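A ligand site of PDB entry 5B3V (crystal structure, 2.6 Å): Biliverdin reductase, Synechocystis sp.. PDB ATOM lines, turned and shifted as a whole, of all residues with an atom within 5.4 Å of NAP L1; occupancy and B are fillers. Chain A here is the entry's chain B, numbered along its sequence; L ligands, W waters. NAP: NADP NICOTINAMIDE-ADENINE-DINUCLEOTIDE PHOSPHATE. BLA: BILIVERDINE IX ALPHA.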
ATOM      1  N   GLY A  20       6.818   2.839  -5.467  1.00  0.00           N
ATOM      2  CA  GLY A  20       5.553   3.548  -5.558  1.00  0.00           C
ATOM      3  C   GLY A  20       4.876   3.333  -6.893  1.00  0.00           C
ATOM      4  O   GLY A  20       5.548   3.001  -7.887  1.00  0.00           O
ATOM      5  N   THR A  21       3.557   3.503  -6.949  1.00  0.00           N
ATOM      6  CA  THR A  21       2.803   3.365  -8.193  1.00  0.00           C
ATOM      7  C   THR A  21       1.841   4.521  -8.435  1.00  0.00           C
ATOM      8  O   THR A  21       0.987   4.415  -9.323  1.00  0.00           O
ATOM      9  CB  THR A  21       2.030   2.042  -8.222  1.00  0.00           C
ATOM     10  OG1 THR A  21       1.125   1.986  -7.105  1.00  0.00           O
ATOM     11  CG2 THR A  21       2.974   0.850  -8.164  1.00  0.00           C
ATOM     12  N   GLY A  22       1.947   5.612  -7.683  1.00  0.00           N
ATOM     13  CA  GLY A  22       1.027   6.721  -7.796  1.00  0.00           C
ATOM     14  C   GLY A  22       1.362   7.652  -8.949  1.00  0.00           C
ATOM     15  O   GLY A  22       2.082   7.300  -9.880  1.00  0.00           O
ATOM     16  N   TYR A  23       0.815   8.871  -8.865  1.00  0.00           N
ATOM     17  CA  TYR A  23       0.949   9.843  -9.948  1.00  0.00           C
ATOM     18  C   TYR A  23       2.418  10.095 -10.295  1.00  0.00           C
ATOM     19  O   TYR A  23       2.828   9.948 -11.449  1.00  0.00           O
ATOM     20  CB  TYR A  23       0.256  11.150  -9.568  1.00  0.00           C
ATOM     21  CG  TYR A  23       0.461  12.253 -10.576  1.00  0.00           C
ATOM     22  CD1 TYR A  23      -0.347  12.353 -11.702  1.00  0.00           C
ATOM     23  CD2 TYR A  23       1.469  13.210 -10.422  1.00  0.00           C
ATOM     24  CE1 TYR A  23      -0.167  13.349 -12.640  1.00  0.00           C
ATOM     25  CE2 TYR A  23       1.656  14.210 -11.349  1.00  0.00           C
ATOM     26  CZ  TYR A  23       0.838  14.284 -12.451  1.00  0.00           C
ATOM     27  OH  TYR A  23       1.019  15.277 -13.381  1.00  0.00           O
ATOM     28  N   ALA A  24       3.211  10.485  -9.292  1.00  0.00           N
ATOM     29  CA  ALA A  24       4.618  10.768  -9.524  1.00  0.00           C
ATOM     30  C   ALA A  24       5.351   9.535 -10.041  1.00  0.00           C
ATOM     31  O   ALA A  24       6.225   9.652 -10.916  1.00  0.00           O
ATOM     32  CB  ALA A  24       5.268  11.274  -8.236  1.00  0.00           C
ATOM     33  N   ALA A  25       5.016   8.361  -9.510  1.00  0.00           N
ATOM     34  CA  ALA A  25       5.679   7.140  -9.961  1.00  0.00           C
ATOM     35  C   ALA A  25       5.397   6.861 -11.427  1.00  0.00           C
ATOM     36  O   ALA A  25       6.247   6.324 -12.141  1.00  0.00           O
ATOM     37  CB  ALA A  25       5.234   5.959  -9.098  1.00  0.00           C
ATOM     38  N   TRP A  44       7.847  -1.399  -6.866  1.00  0.00           N
ATOM     39  CA  TRP A  44       7.156  -1.897  -5.672  1.00  0.00           C
ATOM     40  C   TRP A  44       5.977  -0.988  -5.373  1.00  0.00           C
ATOM     41  O   TRP A  44       6.061   0.230  -5.528  1.00  0.00           O
ATOM     42  CB  TRP A  44       8.106  -1.964  -4.474  1.00  0.00           C
ATOM     43  CG  TRP A  44       7.437  -2.331  -3.199  1.00  0.00           C
ATOM     44  CD1 TRP A  44       7.071  -3.589  -2.794  1.00  0.00           C
ATOM     45  CD2 TRP A  44       7.049  -1.437  -2.149  1.00  0.00           C
ATOM     46  NE1 TRP A  44       6.477  -3.527  -1.556  1.00  0.00           N
ATOM     47  CE2 TRP A  44       6.444  -2.220  -1.138  1.00  0.00           C
ATOM     48  CE3 TRP A  44       7.151  -0.054  -1.962  1.00  0.00           C
ATOM     49  CZ2 TRP A  44       5.952  -1.665   0.041  1.00  0.00           C
ATOM     50  CZ3 TRP A  44       6.659   0.492  -0.798  1.00  0.00           C
ATOM     51  CH2 TRP A  44       6.069  -0.312   0.193  1.00  0.00           C
ATOM     52  N   GLY A  45       4.867  -1.596  -4.931  1.00  0.00           N
ATOM     53  CA  GLY A  45       3.656  -0.835  -4.674  1.00  0.00           C
ATOM     54  C   GLY A  45       2.983  -1.160  -3.351  1.00  0.00           C
ATOM     55  O   GLY A  45       3.635  -1.538  -2.380  1.00  0.00           O
ATOM     56  N   ASN A  46       1.707  -0.889  -3.286  1.00  0.00           N
ATOM     57  CA  ASN A  46       0.921  -1.056  -2.084  1.00  0.00           C
ATOM     58  C   ASN A  46      -0.327  -1.892  -2.286  1.00  0.00           C
ATOM     59  O   ASN A  46      -0.287  -3.034  -2.017  1.00  0.00           O
ATOM     60  CB  ASN A  46       0.666   0.325  -1.474  1.00  0.00           C
ATOM     61  CG  ASN A  46      -0.164   0.278  -0.243  1.00  0.00           C
ATOM     62  OD1 ASN A  46      -1.253   0.782  -0.227  1.00  0.00           O
ATOM     63  ND2 ASN A  46       0.366  -0.283   0.788  1.00  0.00           N
ATOM     64  N   SER A  47      -1.442  -1.316  -2.712  1.00  0.00           N
ATOM     65  CA  SER A  47      -2.659  -2.053  -3.019  1.00  0.00           C
ATOM     66  C   SER A  47      -2.423  -2.982  -4.196  1.00  0.00           C
ATOM     67  O   SER A  47      -1.607  -2.707  -5.080  1.00  0.00           O
ATOM     68  CB  SER A  47      -3.806  -1.085  -3.324  1.00  0.00           C
ATOM     69  OG  SER A  47      -3.814  -0.714  -4.688  1.00  0.00           O
ATOM     70  N   ASN A  50      -3.559  -1.427  -7.818  1.00  0.00           N
ATOM     71  CA  ASN A  50      -2.674  -0.456  -8.452  1.00  0.00           C
ATOM     72  C   ASN A  50      -1.311  -1.037  -8.753  1.00  0.00           C
ATOM     73  O   ASN A  50      -0.629  -0.570  -9.678  1.00  0.00           O
ATOM     74  CB  ASN A  50      -2.548   0.799  -7.586  1.00  0.00           C
ATOM     75  CG  ASN A  50      -3.866   1.516  -7.421  1.00  0.00           C
ATOM     76  OD1 ASN A  50      -4.754   1.414  -8.271  1.00  0.00           O
ATOM     77  ND2 ASN A  50      -4.009   2.259  -6.325  1.00  0.00           N
ATOM     78  N   THR A  51      -0.870  -2.045  -7.991  1.00  0.00           N
ATOM     79  CA  THR A  51       0.343  -2.758  -8.370  1.00  0.00           C
ATOM     80  C   THR A  51       0.145  -3.498  -9.688  1.00  0.00           C
ATOM     81  O   THR A  51       1.064  -3.582 -10.504  1.00  0.00           O
ATOM     82  CB  THR A  51       0.740  -3.727  -7.255  1.00  0.00           C
ATOM     83  OG1 THR A  51       1.404  -3.003  -6.207  1.00  0.00           O
ATOM     84  CG2 THR A  51       1.687  -4.804  -7.777  1.00  0.00           C
ATOM     85  N   ALA A  81       9.146   7.320  -4.830  1.00  0.00           N
ATOM     86  CA  ALA A  81       7.948   8.132  -5.007  1.00  0.00           C
ATOM     87  C   ALA A  81       6.780   7.505  -4.243  1.00  0.00           C
ATOM     88  O   ALA A  81       5.670   7.372  -4.770  1.00  0.00           O
ATOM     89  CB  ALA A  81       7.600   8.286  -6.483  1.00  0.00           C
ATOM     90  N   THR A  82       7.036   7.098  -3.006  1.00  0.00           N
ATOM     91  CA  THR A  82       6.026   6.495  -2.141  1.00  0.00           C
ATOM     92  C   THR A  82       5.668   7.464  -1.022  1.00  0.00           C
ATOM     93  O   THR A  82       6.067   8.632  -1.035  1.00  0.00           O
ATOM     94  CB  THR A  82       6.529   5.153  -1.600  1.00  0.00           C
ATOM     95  OG1 THR A  82       5.544   4.584  -0.737  1.00  0.00           O
ATOM     96  CG2 THR A  82       7.822   5.352  -0.819  1.00  0.00           C
ATOM     97  N   ILE A  83       4.908   6.965  -0.037  1.00  0.00           N
ATOM     98  CA  ILE A  83       4.440   7.836   1.046  1.00  0.00           C
ATOM     99  C   ILE A  83       5.636   8.420   1.791  1.00  0.00           C
ATOM    100  O   ILE A  83       6.704   7.805   1.896  1.00  0.00           O
ATOM    101  CB  ILE A  83       3.515   7.060   1.985  1.00  0.00           C
ATOM    102  CG1 ILE A  83       4.269   5.932   2.679  1.00  0.00           C
ATOM    103  CG2 ILE A  83       2.321   6.507   1.220  1.00  0.00           C
ATOM    104  CD1 ILE A  83       3.515   5.289   3.813  1.00  0.00           C
ATOM    105  N   ASN A  84       5.442   9.641   2.322  1.00  0.00           N
ATOM    106  CA  ASN A  84       6.542  10.393   2.905  1.00  0.00           C
ATOM    107  C   ASN A  84       7.242   9.612   4.018  1.00  0.00           C
ATOM    108  O   ASN A  84       8.470   9.661   4.134  1.00  0.00           O
ATOM    109  CB  ASN A  84       6.039  11.733   3.450  1.00  0.00           C
ATOM    110  CG  ASN A  84       5.610  12.684   2.353  1.00  0.00           C
ATOM    111  OD1 ASN A  84       6.071  12.584   1.212  1.00  0.00           O
ATOM    112  ND2 ASN A  84       4.717  13.609   2.694  1.00  0.00           N
ATOM    113  N   LEU A  86       8.068   6.692   4.468  1.00  0.00           N
ATOM    114  CA  LEU A  86       9.022   5.665   4.072  1.00  0.00           C
ATOM    115  C   LEU A  86      10.261   6.225   3.383  1.00  0.00           C
ATOM    116  O   LEU A  86      11.193   5.461   3.111  1.00  0.00           O
ATOM    117  CB  LEU A  86       8.347   4.646   3.148  1.00  0.00           C
ATOM    118  CG  LEU A  86       7.344   3.701   3.795  1.00  0.00           C
ATOM    119  CD1 LEU A  86       6.810   2.714   2.772  1.00  0.00           C
ATOM    120  CD2 LEU A  86       7.983   2.968   4.964  1.00  0.00           C
ATOM    121  N   HIS A  87      10.298   7.532   3.105  1.00  0.00           N
ATOM    122  CA  HIS A  87      11.425   8.106   2.368  1.00  0.00           C
ATOM    123  C   HIS A  87      12.755   7.841   3.075  1.00  0.00           C
ATOM    124  O   HIS A  87      13.710   7.361   2.458  1.00  0.00           O
ATOM    125  CB  HIS A  87      11.225   9.614   2.171  1.00  0.00           C
ATOM    126  CG  HIS A  87      10.155   9.957   1.188  1.00  0.00           C
ATOM    127  ND1 HIS A  87      10.158  11.149   0.494  1.00  0.00           N
ATOM    128  CD2 HIS A  87       9.061   9.280   0.784  1.00  0.00           C
ATOM    129  CE1 HIS A  87       9.096  11.187  -0.296  1.00  0.00           C
ATOM    130  NE2 HIS A  87       8.421  10.062  -0.141  1.00  0.00           N
ATOM    131  N   GLU A 104      11.304  12.029  -4.529  1.00  0.00           N
ATOM    132  CA  GLU A 104      10.330  13.106  -4.520  1.00  0.00           C
ATOM    133  C   GLU A 104      10.316  13.704  -3.116  1.00  0.00           C
ATOM    134  O   GLU A 104      10.402  12.977  -2.124  1.00  0.00           O
ATOM    135  CB  GLU A 104       8.955  12.563  -4.897  1.00  0.00           C
ATOM    136  CG  GLU A 104       8.551  12.769  -6.347  1.00  0.00           C
ATOM    137  CD  GLU A 104       9.487  12.077  -7.324  1.00  0.00           C
ATOM    138  OE1 GLU A 104       9.412  10.840  -7.446  1.00  0.00           O
ATOM    139  OE2 GLU A 104      10.286  12.779  -7.977  1.00  0.00           O
ATOM    140  N   TYR A 105      10.220  15.028  -3.029  1.00  0.00           N
ATOM    141  CA  TYR A 105      10.294  15.674  -1.723  1.00  0.00           C
ATOM    142  C   TYR A 105       9.119  15.244  -0.840  1.00  0.00           C
ATOM    143  O   TYR A 105       8.058  14.918  -1.350  1.00  0.00           O
ATOM    144  CB  TYR A 105      10.342  17.214  -1.870  1.00  0.00           C
ATOM    145  CG  TYR A 105       9.080  17.888  -2.394  1.00  0.00           C
ATOM    146  CD1 TYR A 105       7.959  18.036  -1.585  1.00  0.00           C
ATOM    147  CD2 TYR A 105       9.040  18.433  -3.666  1.00  0.00           C
ATOM    148  CE1 TYR A 105       6.821  18.668  -2.042  1.00  0.00           C
ATOM    149  CE2 TYR A 105       7.907  19.075  -4.130  1.00  0.00           C
ATOM    150  CZ  TYR A 105       6.806  19.179  -3.319  1.00  0.00           C
ATOM    151  OH  TYR A 105       5.673  19.821  -3.783  1.00  0.00           O
ATOM    152  N   PRO A 106       9.326  15.238   0.492  1.00  0.00           N
ATOM    153  CA  PRO A 106      10.530  15.645   1.222  1.00  0.00           C
ATOM    154  C   PRO A 106      11.625  14.583   1.227  1.00  0.00           C
ATOM    155  O   PRO A 106      11.346  13.402   1.040  1.00  0.00           O
ATOM    156  CB  PRO A 106      10.003  15.868   2.632  1.00  0.00           C
ATOM    157  CG  PRO A 106       8.917  14.864   2.769  1.00  0.00           C
ATOM    158  CD  PRO A 106       8.259  14.814   1.409  1.00  0.00           C
ATOM    159  N   GLU A 131      13.854  15.754  -5.841  1.00  0.00           N
ATOM    160  CA  GLU A 131      13.143  16.493  -6.872  1.00  0.00           C
ATOM    161  C   GLU A 131      12.433  17.696  -6.272  1.00  0.00           C
ATOM    162  O   GLU A 131      11.865  17.618  -5.177  1.00  0.00           O
ATOM    163  CB  GLU A 131      12.152  15.564  -7.577  1.00  0.00           C
ATOM    164  CG  GLU A 131      10.962  16.237  -8.249  1.00  0.00           C
ATOM    165  CD  GLU A 131       9.841  16.551  -7.280  1.00  0.00           C
ATOM    166  OE1 GLU A 131       9.495  15.675  -6.461  1.00  0.00           O
ATOM    167  OE2 GLU A 131       9.314  17.683  -7.318  1.00  0.00           O
ATOM    168  N   ILE A 133      10.030  20.206  -8.287  1.00  0.00           N
ATOM    169  CA  ILE A 133       9.398  20.706  -9.503  1.00  0.00           C
ATOM    170  C   ILE A 133       8.778  22.081  -9.331  1.00  0.00           C
ATOM    171  O   ILE A 133       8.465  22.735 -10.339  1.00  0.00           O
ATOM    172  CB  ILE A 133       8.325  19.723 -10.016  1.00  0.00           C
ATOM    173  CG1 ILE A 133       7.268  19.447  -8.946  1.00  0.00           C
ATOM    174  CG2 ILE A 133       8.976  18.427 -10.495  1.00  0.00           C
ATOM    175  CD1 ILE A 133       6.163  18.514  -9.404  1.00  0.00           C
ATOM    176  N   ARG A 170      -6.931   8.705   2.824  1.00  0.00           N
ATOM    177  CA  ARG A 170      -5.744   8.308   2.085  1.00  0.00           C
ATOM    178  C   ARG A 170      -4.504   8.821   2.809  1.00  0.00           C
ATOM    179  O   ARG A 170      -4.591   9.496   3.841  1.00  0.00           O
ATOM    180  CB  ARG A 170      -5.812   8.831   0.646  1.00  0.00           C
ATOM    181  CG  ARG A 170      -5.468  10.299   0.495  1.00  0.00           C
ATOM    182  CD  ARG A 170      -5.790  10.820  -0.896  1.00  0.00           C
ATOM    183  NE  ARG A 170      -5.105  10.098  -1.966  1.00  0.00           N
ATOM    184  CZ  ARG A 170      -3.901  10.420  -2.431  1.00  0.00           C
ATOM    185  NH1 ARG A 170      -3.243  11.446  -1.933  1.00  0.00           N
ATOM    186  NH2 ARG A 170      -3.356   9.706  -3.407  1.00  0.00           N
ATOM    187  N   TRP A 171      -3.329   8.527   2.250  1.00  0.00           N
ATOM    188  CA  TRP A 171      -2.085   8.754   2.983  1.00  0.00           C
ATOM    189  C   TRP A 171      -1.824  10.244   3.215  1.00  0.00           C
ATOM    190  O   TRP A 171      -1.199  10.612   4.227  1.00  0.00           O
ATOM    191  CB  TRP A 171      -0.915   8.115   2.250  1.00  0.00           C
ATOM    192  CG  TRP A 171      -0.389   8.893   1.073  1.00  0.00           C
ATOM    193  CD1 TRP A 171      -0.818   8.818  -0.214  1.00  0.00           C
ATOM    194  CD2 TRP A 171       0.691   9.844   1.088  1.00  0.00           C
ATOM    195  NE1 TRP A 171      -0.089   9.673  -1.005  1.00  0.00           N
ATOM    196  CE2 TRP A 171       0.837  10.315  -0.232  1.00  0.00           C
ATOM    197  CE3 TRP A 171       1.531  10.359   2.080  1.00  0.00           C
ATOM    198  CZ2 TRP A 171       1.804  11.267  -0.581  1.00  0.00           C
ATOM    199  CZ3 TRP A 171       2.484  11.309   1.732  1.00  0.00           C
ATOM    200  CH2 TRP A 171       2.606  11.746   0.413  1.00  0.00           C
ATOM    201  N   GLN A 177       1.961   8.919   8.069  1.00  0.00           N
ATOM    202  CA  GLN A 177       2.446   8.661   6.714  1.00  0.00           C
ATOM    203  C   GLN A 177       2.696   9.950   5.945  1.00  0.00           C
ATOM    204  O   GLN A 177       3.568   9.976   5.068  1.00  0.00           O
ATOM    205  CB  GLN A 177       1.447   7.781   5.964  1.00  0.00           C
ATOM    206  CG  GLN A 177       1.361   6.357   6.503  1.00  0.00           C
ATOM    207  CD  GLN A 177       0.014   5.708   6.265  1.00  0.00           C
ATOM    208  OE1 GLN A 177      -0.349   4.734   6.920  1.00  0.00           O
ATOM    209  NE2 GLN A 177      -0.739   6.251   5.293  1.00  0.00           N
ATOM    210  N   ALA A 184       5.879  17.985   4.671  1.00  0.00           N
ATOM    211  CA  ALA A 184       5.392  17.272   3.490  1.00  0.00           C
ATOM    212  C   ALA A 184       5.194  18.226   2.316  1.00  0.00           C
ATOM    213  O   ALA A 184       5.558  17.897   1.184  1.00  0.00           O
ATOM    214  CB  ALA A 184       4.085  16.554   3.825  1.00  0.00           C
ATOM    215  N   PHE A 287       8.103  16.770 -14.117  1.00  0.00           N
ATOM    216  CA  PHE A 287       8.709  15.483 -13.781  1.00  0.00           C
ATOM    217  C   PHE A 287       9.655  15.032 -14.881  1.00  0.00           C
ATOM    218  O   PHE A 287      10.737  14.487 -14.600  1.00  0.00           O
ATOM    219  CB  PHE A 287       7.620  14.437 -13.541  1.00  0.00           C
ATOM    220  CG  PHE A 287       7.026  14.498 -12.165  1.00  0.00           C
ATOM    221  CD1 PHE A 287       7.762  14.079 -11.067  1.00  0.00           C
ATOM    222  CD2 PHE A 287       5.743  14.976 -11.966  1.00  0.00           C
ATOM    223  CE1 PHE A 287       7.222  14.127  -9.798  1.00  0.00           C
ATOM    224  CE2 PHE A 287       5.203  15.023 -10.697  1.00  0.00           C
ATOM    225  CZ  PHE A 287       5.946  14.599  -9.602  1.00  0.00           C
HETATM  226  PA  NAP L   1       0.068   8.959  -4.761  1.00  0.00           P
HETATM  227  O1A NAP L   1      -0.369   9.166  -6.164  1.00  0.00           O
HETATM  228  O2A NAP L   1      -0.943   8.757  -3.711  1.00  0.00           O
HETATM  229  O5B NAP L   1       1.042   7.670  -4.776  1.00  0.00           O
HETATM  230  C5B NAP L   1       1.527   6.963  -3.623  1.00  0.00           C
HETATM  231  C4B NAP L   1       1.930   5.494  -3.949  1.00  0.00           C
HETATM  232  O4B NAP L   1       1.436   5.403  -2.566  1.00  0.00           O
HETATM  233  C3B NAP L   1       1.129   4.228  -4.362  1.00  0.00           C
HETATM  234  O3B NAP L   1       2.017   3.109  -4.486  1.00  0.00           O
HETATM  235  C2B NAP L   1       0.297   4.153  -3.120  1.00  0.00           C
HETATM  236  O2B NAP L   1      -0.517   2.967  -2.909  1.00  0.00           O
HETATM  237  C1B NAP L   1       1.516   4.055  -2.209  1.00  0.00           C
HETATM  238  N9A NAP L   1       1.050   3.967  -0.827  1.00  0.00           N
HETATM  239  C8A NAP L   1      -0.078   4.507  -0.373  1.00  0.00           C
HETATM  240  N7A NAP L   1      -0.197   4.187   0.904  1.00  0.00           N
HETATM  241  C5A NAP L   1       0.833   3.414   1.243  1.00  0.00           C
HETATM  242  C6A NAP L   1       1.165   2.835   2.396  1.00  0.00           C
HETATM  243  N6A NAP L   1       0.330   3.058   3.408  1.00  0.00           N
HETATM  244  N1A NAP L   1       2.267   2.086   2.542  1.00  0.00           N
HETATM  245  C2A NAP L   1       3.091   1.902   1.428  1.00  0.00           C
HETATM  246  N3A NAP L   1       2.723   2.515   0.217  1.00  0.00           N
HETATM  247  C4A NAP L   1       1.585   3.244   0.152  1.00  0.00           C
HETATM  248  O3  NAP L   1       0.946  10.245  -4.316  1.00  0.00           O
HETATM  249  PN  NAP L   1       2.052  11.111  -5.121  1.00  0.00           P
HETATM  250  O1N NAP L   1       1.566  12.503  -5.204  1.00  0.00           O
HETATM  251  O2N NAP L   1       2.402  10.370  -6.357  1.00  0.00           O
HETATM  252  O5D NAP L   1       3.329  11.079  -4.148  1.00  0.00           O
HETATM  253  C5D NAP L   1       4.532  10.318  -4.156  1.00  0.00           C
HETATM  254  C4D NAP L   1       5.519  11.007  -3.177  1.00  0.00           C
HETATM  255  O4D NAP L   1       5.225  12.122  -4.128  1.00  0.00           O
HETATM  256  C3D NAP L   1       5.389  12.004  -1.985  1.00  0.00           C
HETATM  257  O3D NAP L   1       6.697  12.346  -1.506  1.00  0.00           O
HETATM  258  C2D NAP L   1       4.782  13.149  -2.698  1.00  0.00           C
HETATM  259  O2D NAP L   1       4.749  14.303  -1.854  1.00  0.00           O
HETATM  260  C1D NAP L   1       5.923  13.272  -3.663  1.00  0.00           C
HETATM  261  N1N NAP L   1       5.637  14.387  -4.594  1.00  0.00           N
HETATM  262  C2N NAP L   1       4.520  14.298  -5.426  1.00  0.00           C
HETATM  263  C3N NAP L   1       4.234  15.331  -6.302  1.00  0.00           C
HETATM  264  C7N NAP L   1       3.138  15.237  -7.138  1.00  0.00           C
HETATM  265  O7N NAP L   1       2.333  14.306  -7.046  1.00  0.00           O
HETATM  266  N7N NAP L   1       3.001  16.236  -8.000  1.00  0.00           N
HETATM  267  C4N NAP L   1       5.073  16.435  -6.397  1.00  0.00           C
HETATM  268  C5N NAP L   1       6.189  16.528  -5.573  1.00  0.00           C
HETATM  269  C6N NAP L   1       6.476  15.501  -4.673  1.00  0.00           C
HETATM  270  P2B NAP L   1      -1.785   2.454  -3.738  1.00  0.00           P
HETATM  271  O1X NAP L   1      -2.658   1.983  -2.665  1.00  0.00           O
HETATM  272  O2X NAP L   1      -2.241   3.640  -4.473  1.00  0.00           O
HETATM  273  O3X NAP L   1      -1.206   1.384  -4.596  1.00  0.00           O
HETATM  274  CHA BLA L   2       2.690  18.913  -5.520  1.00  0.00           C
HETATM  275  NA  BLA L   2       0.852  17.117  -5.555  1.00  0.00           N
HETATM  276  C1A BLA L   2       1.928  17.668  -4.993  1.00  0.00           C
HETATM  277  C2A BLA L   2       2.229  16.992  -3.874  1.00  0.00           C
HETATM  278  C3A BLA L   2       1.362  15.992  -3.780  1.00  0.00           C
HETATM  279  C4A BLA L   2       0.505  16.071  -4.790  1.00  0.00           C
HETATM  280  CMA BLA L   2       1.312  14.940  -2.661  1.00  0.00           C
HETATM  281  CAA BLA L   2       3.399  17.222  -2.896  1.00  0.00           C
HETATM  282  CBA BLA L   2       3.016  17.832  -1.535  1.00  0.00           C
HETATM  283  CGA BLA L   2       2.400  19.231  -1.634  1.00  0.00           C
HETATM  284  O1A BLA L   2       3.147  20.140  -2.073  1.00  0.00           O
HETATM  285  O2A BLA L   2       1.230  19.380  -1.229  1.00  0.00           O
HETATM  286  CHB BLA L   2      -0.666  15.091  -4.990  1.00  0.00           C
HETATM  287  NB  BLA L   2      -1.811  16.652  -6.715  1.00  0.00           N
HETATM  288  C1B BLA L   2      -1.794  15.563  -5.929  1.00  0.00           C
HETATM  289  C2B BLA L   2      -2.929  14.906  -6.105  1.00  0.00           C
HETATM  290  C3B BLA L   2      -3.671  15.558  -6.983  1.00  0.00           C
HETATM  291  C4B BLA L   2      -2.980  16.643  -7.360  1.00  0.00           C
HETATM  292  CMB BLA L   2      -3.330  13.603  -5.401  1.00  0.00           C
HETATM  293  OB  BLA L   2      -3.296  17.635  -8.238  1.00  0.00           O
HETATM  294  CAB BLA L   2      -4.886  15.151  -7.368  1.00  0.00           C
HETATM  295  CBB BLA L   2      -5.634  16.003  -8.405  1.00  0.00           C
HETATM  296  NC  BLA L   2      -0.039  16.627  -9.233  1.00  0.00           N
HETATM  297  C1C BLA L   2      -0.955  15.722  -9.549  1.00  0.00           C
HETATM  298  C2C BLA L   2      -1.549  16.077 -10.696  1.00  0.00           C
HETATM  299  C3C BLA L   2      -0.982  17.221 -11.103  1.00  0.00           C
HETATM  300  C4C BLA L   2      -0.064  17.546 -10.191  1.00  0.00           C
HETATM  301  CMC BLA L   2      -2.667  15.220 -11.328  1.00  0.00           C
HETATM  302  OC  BLA L   2      -1.211  14.638  -8.777  1.00  0.00           O
HETATM  303  CAC BLA L   2      -1.181  18.013 -12.177  1.00  0.00           C
HETATM  304  CBC BLA L   2      -2.209  17.641 -13.256  1.00  0.00           C
HETATM  305  CHD BLA L   2       0.819  18.802 -10.286  1.00  0.00           C
HETATM  306  ND  BLA L   2       1.550  18.589  -7.796  1.00  0.00           N
HETATM  307  C1D BLA L   2       1.610  19.151  -9.007  1.00  0.00           C
HETATM  308  C2D BLA L   2       2.494  20.136  -8.959  1.00  0.00           C
HETATM  309  C3D BLA L   2       3.008  20.188  -7.744  1.00  0.00           C
HETATM  310  C4D BLA L   2       2.427  19.226  -7.008  1.00  0.00           C
HETATM  311  CMD BLA L   2       2.874  21.049 -10.133  1.00  0.00           C
HETATM  312  CAD BLA L   2       4.067  21.221  -7.361  1.00  0.00           C
HETATM  313  CBD BLA L   2       3.381  22.291  -6.513  1.00  0.00           C
HETATM  314  CGD BLA L   2       4.295  23.446  -6.133  1.00  0.00           C
HETATM  315  O1D BLA L   2       4.819  24.064  -7.081  1.00  0.00           O
HETATM  316  O2D BLA L   2       4.390  23.742  -4.921  1.00  0.00           O
HETATM  317  O   HOH W   1       4.171  15.218   0.516  1.00  0.00           O
HETATM  318  O   HOH W   2       4.383   2.528  -2.158  1.00  0.00           O
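The backbone NH (N) of Asn 84 is in hydrogen-bond range of the backbone carbonyl oxygen (O) of Gln 177 (3.3 Å). OG of Ser 47 is in hydrogen-bond range of N of Asn 50, 3.2 Å away. NE2 of His 87 lies within hydrogen-bond range of O of Thr 82, 2.9 Å away. ND1 of His 87 lies close to O of Glu 104, at 3.2 Å. ND1 of His 87 is in hydrogen-bond range of O of Pro 106 (2.6 Å). The side-chain hydroxyl (OG1) of Thr 51 sits at hydrogen-bond distance from the backbone carbonyl oxygen (O) of Ser 47. OE2 of Glu 131 sits at hydrogen-bond distance from N of Ile 133 (2.8 Å). O of Trp 44 is in hydrogen-bond range of N of Gly 20.
A nitrogen (ND) of BLA L2 is in hydrogen-bond range of a nitrogen (N7N) of NAP L1 (2.8 Å).
NH2 of Arg 170 is in salt-bridge range of O2A of NAP L1. The side-chain amide oxygen (OD1) of Asn 84 sits at hydrogen-bond distance from an oxygen (O3D) of NAP L1 (2.8 Å). ND2 of Asn 50 is in hydrogen-bond range of O2X of NAP L1 (2.9 Å). The backbone carbonyl oxygen (O) of Tyr 105 is in hydrogen-bond range of an oxygen (O3D) of NAP L1, at 2.9 Å. NE2 of His 87 sits close to O3D of NAP L1. An oxygen (O3B) of NAP L1 is in hydrogen-bond range of the backbone NH of Thr 21 (2.9 Å). The side-chain hydroxyl (OG1) of Thr 21 is in hydrogen-bond range of an oxygen (O3B) of NAP L1, at 3.0 Å. An oxygen (O1A) of NAP L1 lies within hydrogen-bond range of the backbone NH (N) of Tyr 23 (3.0 Å). O2A of NAP L1 sits at hydrogen-bond distance from NE1 of Trp 171 (3.0 Å). N of Ala 24 sits at hydrogen-bond distance from O2N of NAP L1 (3.0 Å). The side-chain amide oxygen (OD1) of Asn 46 sits close to an oxygen (O1X) of NAP L1 (3.1 Å). The backbone NH (N) of Ser 47 is in hydrogen-bond range of an oxygen (O3X) of NAP L1. The side-chain hydroxyl (OG) of Ser 47 lies within hydrogen-bond range of an oxygen (O3X) of NAP L1, 3.3 Å away. The side-chain hydroxyl of Tyr 105 sits at hydrogen-bond distance from an oxygen (O1A) of BLA L2, at 3.1 Å.
Water W1 lies within hydrogen-bond range of O2D of NAP L1 (2.6 Å), ND2 of Asn 84 (2.8 Å) and O of Ala 184 (3.1 Å). Water W2 bridges the side-chain hydroxyl of Thr 82 (2.8 Å) and a nitrogen (N3A) of NAP L1 (2.9 Å).
Merely in contact with NAP L1: Gly 20 (3.7 Å), Gly 22 (3.2 Å), Trp 44 (3.9 Å), Ala 81 (3.2 Å), Thr 82 (3.2 Å), Ile 83 (3.4 Å), Glu 104 (3.3 Å), Glu 131 (3.5 Å), Ile 133 (3.8 Å), Gln 177 (3.9 Å) and Phe 287 (3.7 Å). Hydrophobic or aromatic side chains that line NAP L1: Tyr 23, Ala 24, Trp 44, Ile 83, His 87, Tyr 105, Ile 133, Trp 171 and Phe 287. Within 4 Å of NAP L1: Gly 20, Thr 21, Gly 22, Tyr 23, Ala 24, Trp 44, Asn 46, Ser 47, Asn 50, Ala 81, Thr 82, Ile 83, Asn 84, His 87, Glu 104, Tyr 105, Glu 131, Ile 133, Arg 170, Trp 171, Gln 177 and Phe 287. Along chain A the residues within 4 Å of NAP L1 span positions 20 to 287.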
